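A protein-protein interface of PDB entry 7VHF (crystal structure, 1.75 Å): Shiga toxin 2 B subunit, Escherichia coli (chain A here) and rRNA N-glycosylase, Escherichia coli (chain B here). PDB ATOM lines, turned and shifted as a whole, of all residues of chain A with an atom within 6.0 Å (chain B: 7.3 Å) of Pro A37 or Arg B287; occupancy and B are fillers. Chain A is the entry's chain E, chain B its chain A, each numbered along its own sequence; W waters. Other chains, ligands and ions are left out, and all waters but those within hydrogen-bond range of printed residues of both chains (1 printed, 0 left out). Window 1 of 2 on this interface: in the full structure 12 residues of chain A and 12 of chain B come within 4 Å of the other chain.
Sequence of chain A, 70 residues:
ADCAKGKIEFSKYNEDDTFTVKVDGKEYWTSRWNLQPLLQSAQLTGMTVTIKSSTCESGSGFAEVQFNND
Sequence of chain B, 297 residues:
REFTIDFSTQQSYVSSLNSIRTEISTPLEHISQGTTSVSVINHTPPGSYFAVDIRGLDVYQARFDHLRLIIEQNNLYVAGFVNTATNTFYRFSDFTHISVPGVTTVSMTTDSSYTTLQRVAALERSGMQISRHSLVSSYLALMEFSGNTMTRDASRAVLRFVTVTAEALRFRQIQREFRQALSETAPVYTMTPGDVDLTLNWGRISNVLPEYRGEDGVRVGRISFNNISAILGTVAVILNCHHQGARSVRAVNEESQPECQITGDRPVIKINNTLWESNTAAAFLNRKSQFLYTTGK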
ATOM      1  N   TRP A  33      -9.383   9.294 -18.851  1.00  0.00           N
ATOM      2  CA  TRP A  33      -8.993  10.643 -18.460  1.00  0.00           C
ATOM      3  C   TRP A  33      -9.555  10.993 -17.094  1.00  0.00           C
ATOM      4  O   TRP A  33      -8.948  11.786 -16.367  1.00  0.00           O
ATOM      5  CB  TRP A  33      -9.448  11.664 -19.503  1.00  0.00           C
ATOM      6  CG  TRP A  33      -8.498  11.811 -20.670  1.00  0.00           C
ATOM      7  CD1 TRP A  33      -7.632  10.870 -21.157  1.00  0.00           C
ATOM      8  CD2 TRP A  33      -8.341  12.970 -21.495  1.00  0.00           C
ATOM      9  NE1 TRP A  33      -6.941  11.383 -22.246  1.00  0.00           N
ATOM     10  CE2 TRP A  33      -7.358  12.670 -22.464  1.00  0.00           C
ATOM     11  CE3 TRP A  33      -8.926  14.236 -21.504  1.00  0.00           C
ATOM     12  CZ2 TRP A  33      -6.950  13.599 -23.433  1.00  0.00           C
ATOM     13  CZ3 TRP A  33      -8.525  15.152 -22.470  1.00  0.00           C
ATOM     14  CH2 TRP A  33      -7.551  14.827 -23.419  1.00  0.00           C
ATOM     15  N   ASN A  34     -10.707  10.413 -16.722  1.00  0.00           N
ATOM     16  CA  ASN A  34     -11.234  10.640 -15.378  1.00  0.00           C
ATOM     17  C   ASN A  34     -10.158  10.408 -14.332  1.00  0.00           C
ATOM     18  O   ASN A  34     -10.111  11.103 -13.313  1.00  0.00           O
ATOM     19  CB  ASN A  34     -12.409   9.699 -15.072  1.00  0.00           C
ATOM     20  CG  ASN A  34     -13.719  10.164 -15.662  1.00  0.00           C
ATOM     21  OD1 ASN A  34     -13.894  11.338 -15.988  1.00  0.00           O
ATOM     22  ND2 ASN A  34     -14.654   9.225 -15.817  1.00  0.00           N
ATOM     23  N   LEU A  35      -9.288   9.427 -14.565  1.00  0.00           N
ATOM     24  CA  LEU A  35      -8.325   9.052 -13.540  1.00  0.00           C
ATOM     25  C   LEU A  35      -7.114   9.972 -13.489  1.00  0.00           C
ATOM     26  O   LEU A  35      -6.393   9.951 -12.487  1.00  0.00           O
ATOM     27  CB  LEU A  35      -7.875   7.603 -13.760  1.00  0.00           C
ATOM     28  CG  LEU A  35      -8.863   6.614 -13.140  1.00  0.00           C
ATOM     29  CD1 LEU A  35      -8.528   5.192 -13.549  1.00  0.00           C
ATOM     30  CD2 LEU A  35      -8.823   6.762 -11.621  1.00  0.00           C
ATOM     31  N   GLN A  36      -6.875  10.797 -14.516  1.00  0.00           N
ATOM     32  CA  GLN A  36      -5.671  11.627 -14.478  1.00  0.00           C
ATOM     33  C   GLN A  36      -5.690  12.632 -13.332  1.00  0.00           C
ATOM     34  O   GLN A  36      -4.735  12.635 -12.530  1.00  0.00           O
ATOM     35  CB  GLN A  36      -5.447  12.298 -15.837  1.00  0.00           C
ATOM     36  CG  GLN A  36      -5.216  11.295 -16.945  1.00  0.00           C
ATOM     37  CD  GLN A  36      -4.669  11.934 -18.200  1.00  0.00           C
ATOM     38  OE1 GLN A  36      -4.157  13.062 -18.168  1.00  0.00           O
ATOM     39  NE2 GLN A  36      -4.764  11.214 -19.315  1.00  0.00           N
ATOM     40  N   PRO A  37      -6.712  13.482 -13.169  1.00  0.00           N
ATOM     41  CA  PRO A  37      -6.696  14.385 -12.002  1.00  0.00           C
ATOM     42  C   PRO A  37      -6.753  13.625 -10.694  1.00  0.00           C
ATOM     43  O   PRO A  37      -6.023  13.953  -9.754  1.00  0.00           O
ATOM     44  CB  PRO A  37      -7.942  15.260 -12.205  1.00  0.00           C
ATOM     45  CG  PRO A  37      -8.797  14.509 -13.199  1.00  0.00           C
ATOM     46  CD  PRO A  37      -7.852  13.755 -14.065  1.00  0.00           C
ATOM     47  N   LEU A  38      -7.569  12.568 -10.636  1.00  0.00           N
ATOM     48  CA  LEU A  38      -7.693  11.790  -9.404  1.00  0.00           C
ATOM     49  C   LEU A  38      -6.349  11.223  -8.982  1.00  0.00           C
ATOM     50  O   LEU A  38      -5.946  11.345  -7.818  1.00  0.00           O
ATOM     51  CB  LEU A  38      -8.712  10.668  -9.598  1.00  0.00           C
ATOM     52  CG  LEU A  38     -10.094  11.129 -10.021  1.00  0.00           C
ATOM     53  CD1 LEU A  38     -10.978   9.907 -10.225  1.00  0.00           C
ATOM     54  CD2 LEU A  38     -10.680  12.024  -8.954  1.00  0.00           C
ATOM     55  N   LEU A  39      -5.622  10.638  -9.935  1.00  0.00           N
ATOM     56  CA  LEU A  39      -4.326  10.060  -9.628  1.00  0.00           C
ATOM     57  C   LEU A  39      -3.314  11.150  -9.313  1.00  0.00           C
ATOM     58  O   LEU A  39      -2.529  11.020  -8.366  1.00  0.00           O
ATOM     59  CB  LEU A  39      -3.861   9.178 -10.794  1.00  0.00           C
ATOM     60  CG  LEU A  39      -4.562   7.818 -10.974  1.00  0.00           C
ATOM     61  CD1 LEU A  39      -4.216   7.178 -12.311  1.00  0.00           C
ATOM     62  CD2 LEU A  39      -4.199   6.862  -9.828  1.00  0.00           C
ATOM     63  N   GLN A  40      -3.346  12.266 -10.051  1.00  0.00           N
ATOM     64  CA  GLN A  40      -2.302  13.251  -9.785  1.00  0.00           C
ATOM     65  C   GLN A  40      -2.520  13.900  -8.430  1.00  0.00           C
ATOM     66  O   GLN A  40      -1.565  14.118  -7.673  1.00  0.00           O
ATOM     67  CB  GLN A  40      -2.237  14.306 -10.885  1.00  0.00           C
ATOM     68  CG  GLN A  40      -0.997  15.181 -10.664  1.00  0.00           C
ATOM     69  CD  GLN A  40      -1.109  16.539 -11.287  1.00  0.00           C
ATOM     70  OE1 GLN A  40      -2.128  17.222 -11.143  1.00  0.00           O
ATOM     71  NE2 GLN A  40      -0.045  16.962 -11.965  1.00  0.00           N
ATOM     72  N   SER A  41      -3.772  14.209  -8.105  1.00  0.00           N
ATOM     73  CA  SER A  41      -4.073  14.675  -6.759  1.00  0.00           C
ATOM     74  C   SER A  41      -3.623  13.658  -5.721  1.00  0.00           C
ATOM     75  O   SER A  41      -2.998  14.027  -4.717  1.00  0.00           O
ATOM     76  CB  SER A  41      -5.566  14.980  -6.621  1.00  0.00           C
ATOM     77  OG  SER A  41      -5.925  16.044  -7.484  1.00  0.00           O
ATOM     78  N   ALA A  42      -3.886  12.367  -5.968  1.00  0.00           N
ATOM     79  CA  ALA A  42      -3.416  11.357  -5.027  1.00  0.00           C
ATOM     80  C   ALA A  42      -1.903  11.422  -4.905  1.00  0.00           C
ATOM     81  O   ALA A  42      -1.352  11.315  -3.808  1.00  0.00           O
ATOM     82  CB  ALA A  42      -3.871   9.963  -5.470  1.00  0.00           C
ATOM     83  N   LEU A  44       0.062  14.088  -5.348  1.00  0.00           N
ATOM     84  CA  LEU A  44       0.653  15.275  -4.758  1.00  0.00           C
ATOM     85  C   LEU A  44       0.267  15.428  -3.300  1.00  0.00           C
ATOM     86  O   LEU A  44       0.917  16.193  -2.582  1.00  0.00           O
ATOM     87  CB  LEU A  44       0.262  16.523  -5.554  1.00  0.00           C
ATOM     88  CG  LEU A  44      -1.187  16.989  -5.626  1.00  0.00           C
ATOM     89  CD1 LEU A  44      -1.439  18.049  -4.573  1.00  0.00           C
ATOM     90  CD2 LEU A  44      -1.456  17.576  -7.012  1.00  0.00           C
ATOM     91  N   ALA B 282      -4.600  24.255  -3.560  1.00  0.00           N
ATOM     92  CA  ALA B 282      -4.797  24.827  -4.889  1.00  0.00           C
ATOM     93  C   ALA B 282      -4.585  23.783  -5.974  1.00  0.00           C
ATOM     94  O   ALA B 282      -5.304  23.770  -6.978  1.00  0.00           O
ATOM     95  CB  ALA B 282      -3.848  26.016  -5.100  1.00  0.00           C
ATOM     96  N   ALA B 283      -3.614  22.883  -5.782  1.00  0.00           N
ATOM     97  CA  ALA B 283      -3.286  21.899  -6.803  1.00  0.00           C
ATOM     98  C   ALA B 283      -4.298  20.769  -6.922  1.00  0.00           C
ATOM     99  O   ALA B 283      -4.241  20.040  -7.916  1.00  0.00           O
ATOM    100  CB  ALA B 283      -1.899  21.304  -6.543  1.00  0.00           C
ATOM    101  N   PHE B 284      -5.205  20.571  -5.958  1.00  0.00           N
ATOM    102  CA  PHE B 284      -6.329  19.681  -6.262  1.00  0.00           C
ATOM    103  C   PHE B 284      -7.678  20.395  -6.356  1.00  0.00           C
ATOM    104  O   PHE B 284      -8.694  19.739  -6.597  1.00  0.00           O
ATOM    105  CB  PHE B 284      -6.399  18.492  -5.279  1.00  0.00           C
ATOM    106  CG  PHE B 284      -6.655  18.853  -3.826  1.00  0.00           C
ATOM    107  CD1 PHE B 284      -7.945  19.059  -3.353  1.00  0.00           C
ATOM    108  CD2 PHE B 284      -5.609  18.865  -2.913  1.00  0.00           C
ATOM    109  CE1 PHE B 284      -8.185  19.336  -1.999  1.00  0.00           C
ATOM    110  CE2 PHE B 284      -5.837  19.137  -1.553  1.00  0.00           C
ATOM    111  CZ  PHE B 284      -7.118  19.370  -1.097  1.00  0.00           C
ATOM    112  N   LEU B 285      -7.707  21.724  -6.253  1.00  0.00           N
ATOM    113  CA  LEU B 285      -8.926  22.497  -6.435  1.00  0.00           C
ATOM    114  C   LEU B 285      -8.917  23.259  -7.756  1.00  0.00           C
ATOM    115  O   LEU B 285      -9.688  24.207  -7.931  1.00  0.00           O
ATOM    116  CB  LEU B 285      -9.116  23.461  -5.264  1.00  0.00           C
ATOM    117  CG  LEU B 285      -9.225  22.761  -3.905  1.00  0.00           C
ATOM    118  CD1 LEU B 285      -9.234  23.771  -2.759  1.00  0.00           C
ATOM    119  CD2 LEU B 285     -10.490  21.906  -3.872  1.00  0.00           C
ATOM    120  N   ASN B 286      -8.048  22.877  -8.686  1.00  0.00           N
ATOM    121  CA  ASN B 286      -7.954  23.564  -9.967  1.00  0.00           C
ATOM    122  C   ASN B 286      -8.505  22.721 -11.110  1.00  0.00           C
ATOM    123  O   ASN B 286      -8.140  22.947 -12.263  1.00  0.00           O
ATOM    124  CB  ASN B 286      -6.506  23.965 -10.262  1.00  0.00           C
ATOM    125  CG  ASN B 286      -5.606  22.769 -10.473  1.00  0.00           C
ATOM    126  OD1 ASN B 286      -5.982  21.637 -10.158  1.00  0.00           O
ATOM    127  ND2 ASN B 286      -4.407  23.008 -11.004  1.00  0.00           N
ATOM    128  N   ARG B 287      -9.368  21.748 -10.809  1.00  0.00           N
ATOM    129  CA  ARG B 287      -9.955  20.884 -11.823  1.00  0.00           C
ATOM    130  C   ARG B 287     -11.299  21.448 -12.253  1.00  0.00           C
ATOM    131  O   ARG B 287     -12.068  21.932 -11.424  1.00  0.00           O
ATOM    132  CB  ARG B 287     -10.138  19.465 -11.283  1.00  0.00           C
ATOM    133  CG  ARG B 287      -8.857  18.625 -11.243  1.00  0.00           C
ATOM    134  CD  ARG B 287      -7.969  18.957 -10.041  1.00  0.00           C
ATOM    135  NE  ARG B 287      -6.945  17.937  -9.873  1.00  0.00           N
ATOM    136  CZ  ARG B 287      -5.696  18.013 -10.318  1.00  0.00           C
ATOM    137  NH1 ARG B 287      -5.245  19.083 -10.957  1.00  0.00           N
ATOM    138  NH2 ARG B 287      -4.876  16.982 -10.116  1.00  0.00           N
ATOM    139  N   LYS B 288     -11.579  21.387 -13.550  1.00  0.00           N
ATOM    140  CA  LYS B 288     -12.901  21.786 -14.004  1.00  0.00           C
ATOM    141  C   LYS B 288     -13.850  20.596 -13.901  1.00  0.00           C
ATOM    142  O   LYS B 288     -13.506  19.529 -13.384  1.00  0.00           O
ATOM    143  CB  LYS B 288     -12.857  22.343 -15.424  1.00  0.00           C
ATOM    144  CG  LYS B 288     -12.636  21.308 -16.505  1.00  0.00           C
ATOM    145  CD  LYS B 288     -12.711  21.978 -17.887  1.00  0.00           C
ATOM    146  CE  LYS B 288     -12.475  20.987 -19.011  1.00  0.00           C
ATOM    147  NZ  LYS B 288     -12.571  21.650 -20.343  1.00  0.00           N
ATOM    148  N   SER B 289     -15.074  20.794 -14.368  1.00  0.00           N
ATOM    149  CA  SER B 289     -16.082  19.747 -14.275  1.00  0.00           C
ATOM    150  C   SER B 289     -15.580  18.479 -14.950  1.00  0.00           C
ATOM    151  O   SER B 289     -15.094  18.507 -16.086  1.00  0.00           O
ATOM    152  CB  SER B 289     -17.385  20.221 -14.911  1.00  0.00           C
ATOM    153  OG  SER B 289     -18.251  19.122 -15.156  1.00  0.00           O
ATOM    154  N   GLN B 290     -15.694  17.364 -14.235  1.00  0.00           N
ATOM    155  CA  GLN B 290     -15.068  16.126 -14.676  1.00  0.00           C
ATOM    156  C   GLN B 290     -15.617  15.646 -16.015  1.00  0.00           C
ATOM    157  O   GLN B 290     -14.849  15.217 -16.883  1.00  0.00           O
ATOM    158  CB  GLN B 290     -15.260  15.063 -13.599  1.00  0.00           C
ATOM    159  CG  GLN B 290     -14.618  13.731 -13.891  1.00  0.00           C
ATOM    160  CD  GLN B 290     -13.158  13.696 -13.506  1.00  0.00           C
ATOM    161  OE1 GLN B 290     -12.420  14.673 -13.703  1.00  0.00           O
ATOM    162  NE2 GLN B 290     -12.720  12.558 -12.964  1.00  0.00           N
ATOM    163  N   TYR B 293     -14.082  17.749 -18.622  1.00  0.00           N
ATOM    164  CA  TYR B 293     -12.664  17.436 -18.763  1.00  0.00           C
ATOM    165  C   TYR B 293     -12.467  16.183 -19.597  1.00  0.00           C
ATOM    166  O   TYR B 293     -11.708  16.172 -20.578  1.00  0.00           O
ATOM    167  CB  TYR B 293     -12.044  17.248 -17.381  1.00  0.00           C
ATOM    168  CG  TYR B 293     -10.599  16.800 -17.382  1.00  0.00           C
ATOM    169  CD1 TYR B 293      -9.567  17.704 -17.616  1.00  0.00           C
ATOM    170  CD2 TYR B 293     -10.267  15.481 -17.082  1.00  0.00           C
ATOM    171  CE1 TYR B 293      -8.237  17.292 -17.580  1.00  0.00           C
ATOM    172  CE2 TYR B 293      -8.953  15.066 -17.036  1.00  0.00           C
ATOM    173  CZ  TYR B 293      -7.943  15.971 -17.280  1.00  0.00           C
ATOM    174  OH  TYR B 293      -6.629  15.556 -17.234  1.00  0.00           O
ATOM    175  N   THR B 294     -13.165  15.115 -19.234  1.00  0.00           N
ATOM    176  CA  THR B 294     -12.873  13.830 -19.844  1.00  0.00           C
ATOM    177  C   THR B 294     -13.405  13.757 -21.266  1.00  0.00           C
ATOM    178  O   THR B 294     -12.791  13.103 -22.120  1.00  0.00           O
ATOM    179  CB  THR B 294     -13.440  12.722 -18.961  1.00  0.00           C
ATOM    180  OG1 THR B 294     -12.738  12.751 -17.711  1.00  0.00           O
ATOM    181  CG2 THR B 294     -13.303  11.343 -19.625  1.00  0.00           C
HETATM  182  O   HOH W   1      -8.656  15.876  -8.157  1.00  0.00           O
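Of the 11 printed residues of chain A, 7 touch a printed residue of chain B. Of the 11 printed residues of chain B, 6 touch a printed residue of chain A. Hydrophobic or aromatic side chains of chain B that line the printed part of chain A: Ala B283, Phe B284 and Tyr B293. Among the printed residues, no Asp or Glu carboxylate lies within 4 Å of a Lys or Arg side-chain nitrogen of the other chain.
The backbone carbonyl oxygen of Ala B283 lies within hydrogen-bond range of the guanidinium group of Arg B287. The backbone carbonyl oxygen of Ala B283 sits close to the side-chain amide oxygen of Asn B286 (3.3 Å). The guanidinium group (NH1) of Arg B287 is in hydrogen-bond range of the side-chain amide oxygen (OD1) of Asn B286 (2.8 Å). O of Pro A37 sits at hydrogen-bond distance from OG of Ser A41 (3.1 Å). The backbone carbonyl oxygen (O) of Gln B290 lies within hydrogen-bond range of the side-chain hydroxyl (OG1) of Thr B294 (3.4 Å).
The backbone carbonyl oxygen (O) of Asn A34 is in hydrogen-bond range of the side-chain amide nitrogen (NE2) of Gln B290 (3.0 Å). The side-chain hydroxyl (OG1) of Thr B294 lies within hydrogen-bond range of the side-chain amide oxygen (OD1) of Asn A34 (2.5 Å). The guanidinium group (NH2) of Arg B287 sits at hydrogen-bond distance from the backbone carbonyl oxygen (O) of Pro A37 (3.3 Å). The guanidinium group (NH2) of Arg B287 lies within hydrogen-bond range of the side-chain amide oxygen (OE1) of Gln A40. The guanidinium group (NH2) of Arg B287 sits at hydrogen-bond distance from the side-chain hydroxyl (OG) of Ser A41 (3.0 Å).
Water W1 lies within hydrogen-bond range of OG of Ser A41 (2.8 Å) and NE of Arg B287 (3.2 Å).
Arg B287 touches three residues of chain A. Printed residues of chain A within 4 Å of Gln B290: Asn A34 (3.0 Å) and Pro A37 (3.7 Å). Printed residues of chain B within 4 Å of Gln A36: Tyr B293 (3.6 Å). Leu A35 touches none of the printed residues of chain B. Ala B282 touches none of the printed residues of chain A.
Among the printed residues, pairs that only touch across the chains: Trp A33 with Tyr B293, Trp A33 with Thr B294, Gln A36 with Tyr B293, Pro A37 with Gln B290, Pro A37 with Tyr B293, Ser A41 with Phe B284 and Leu A44 with Ala B283.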
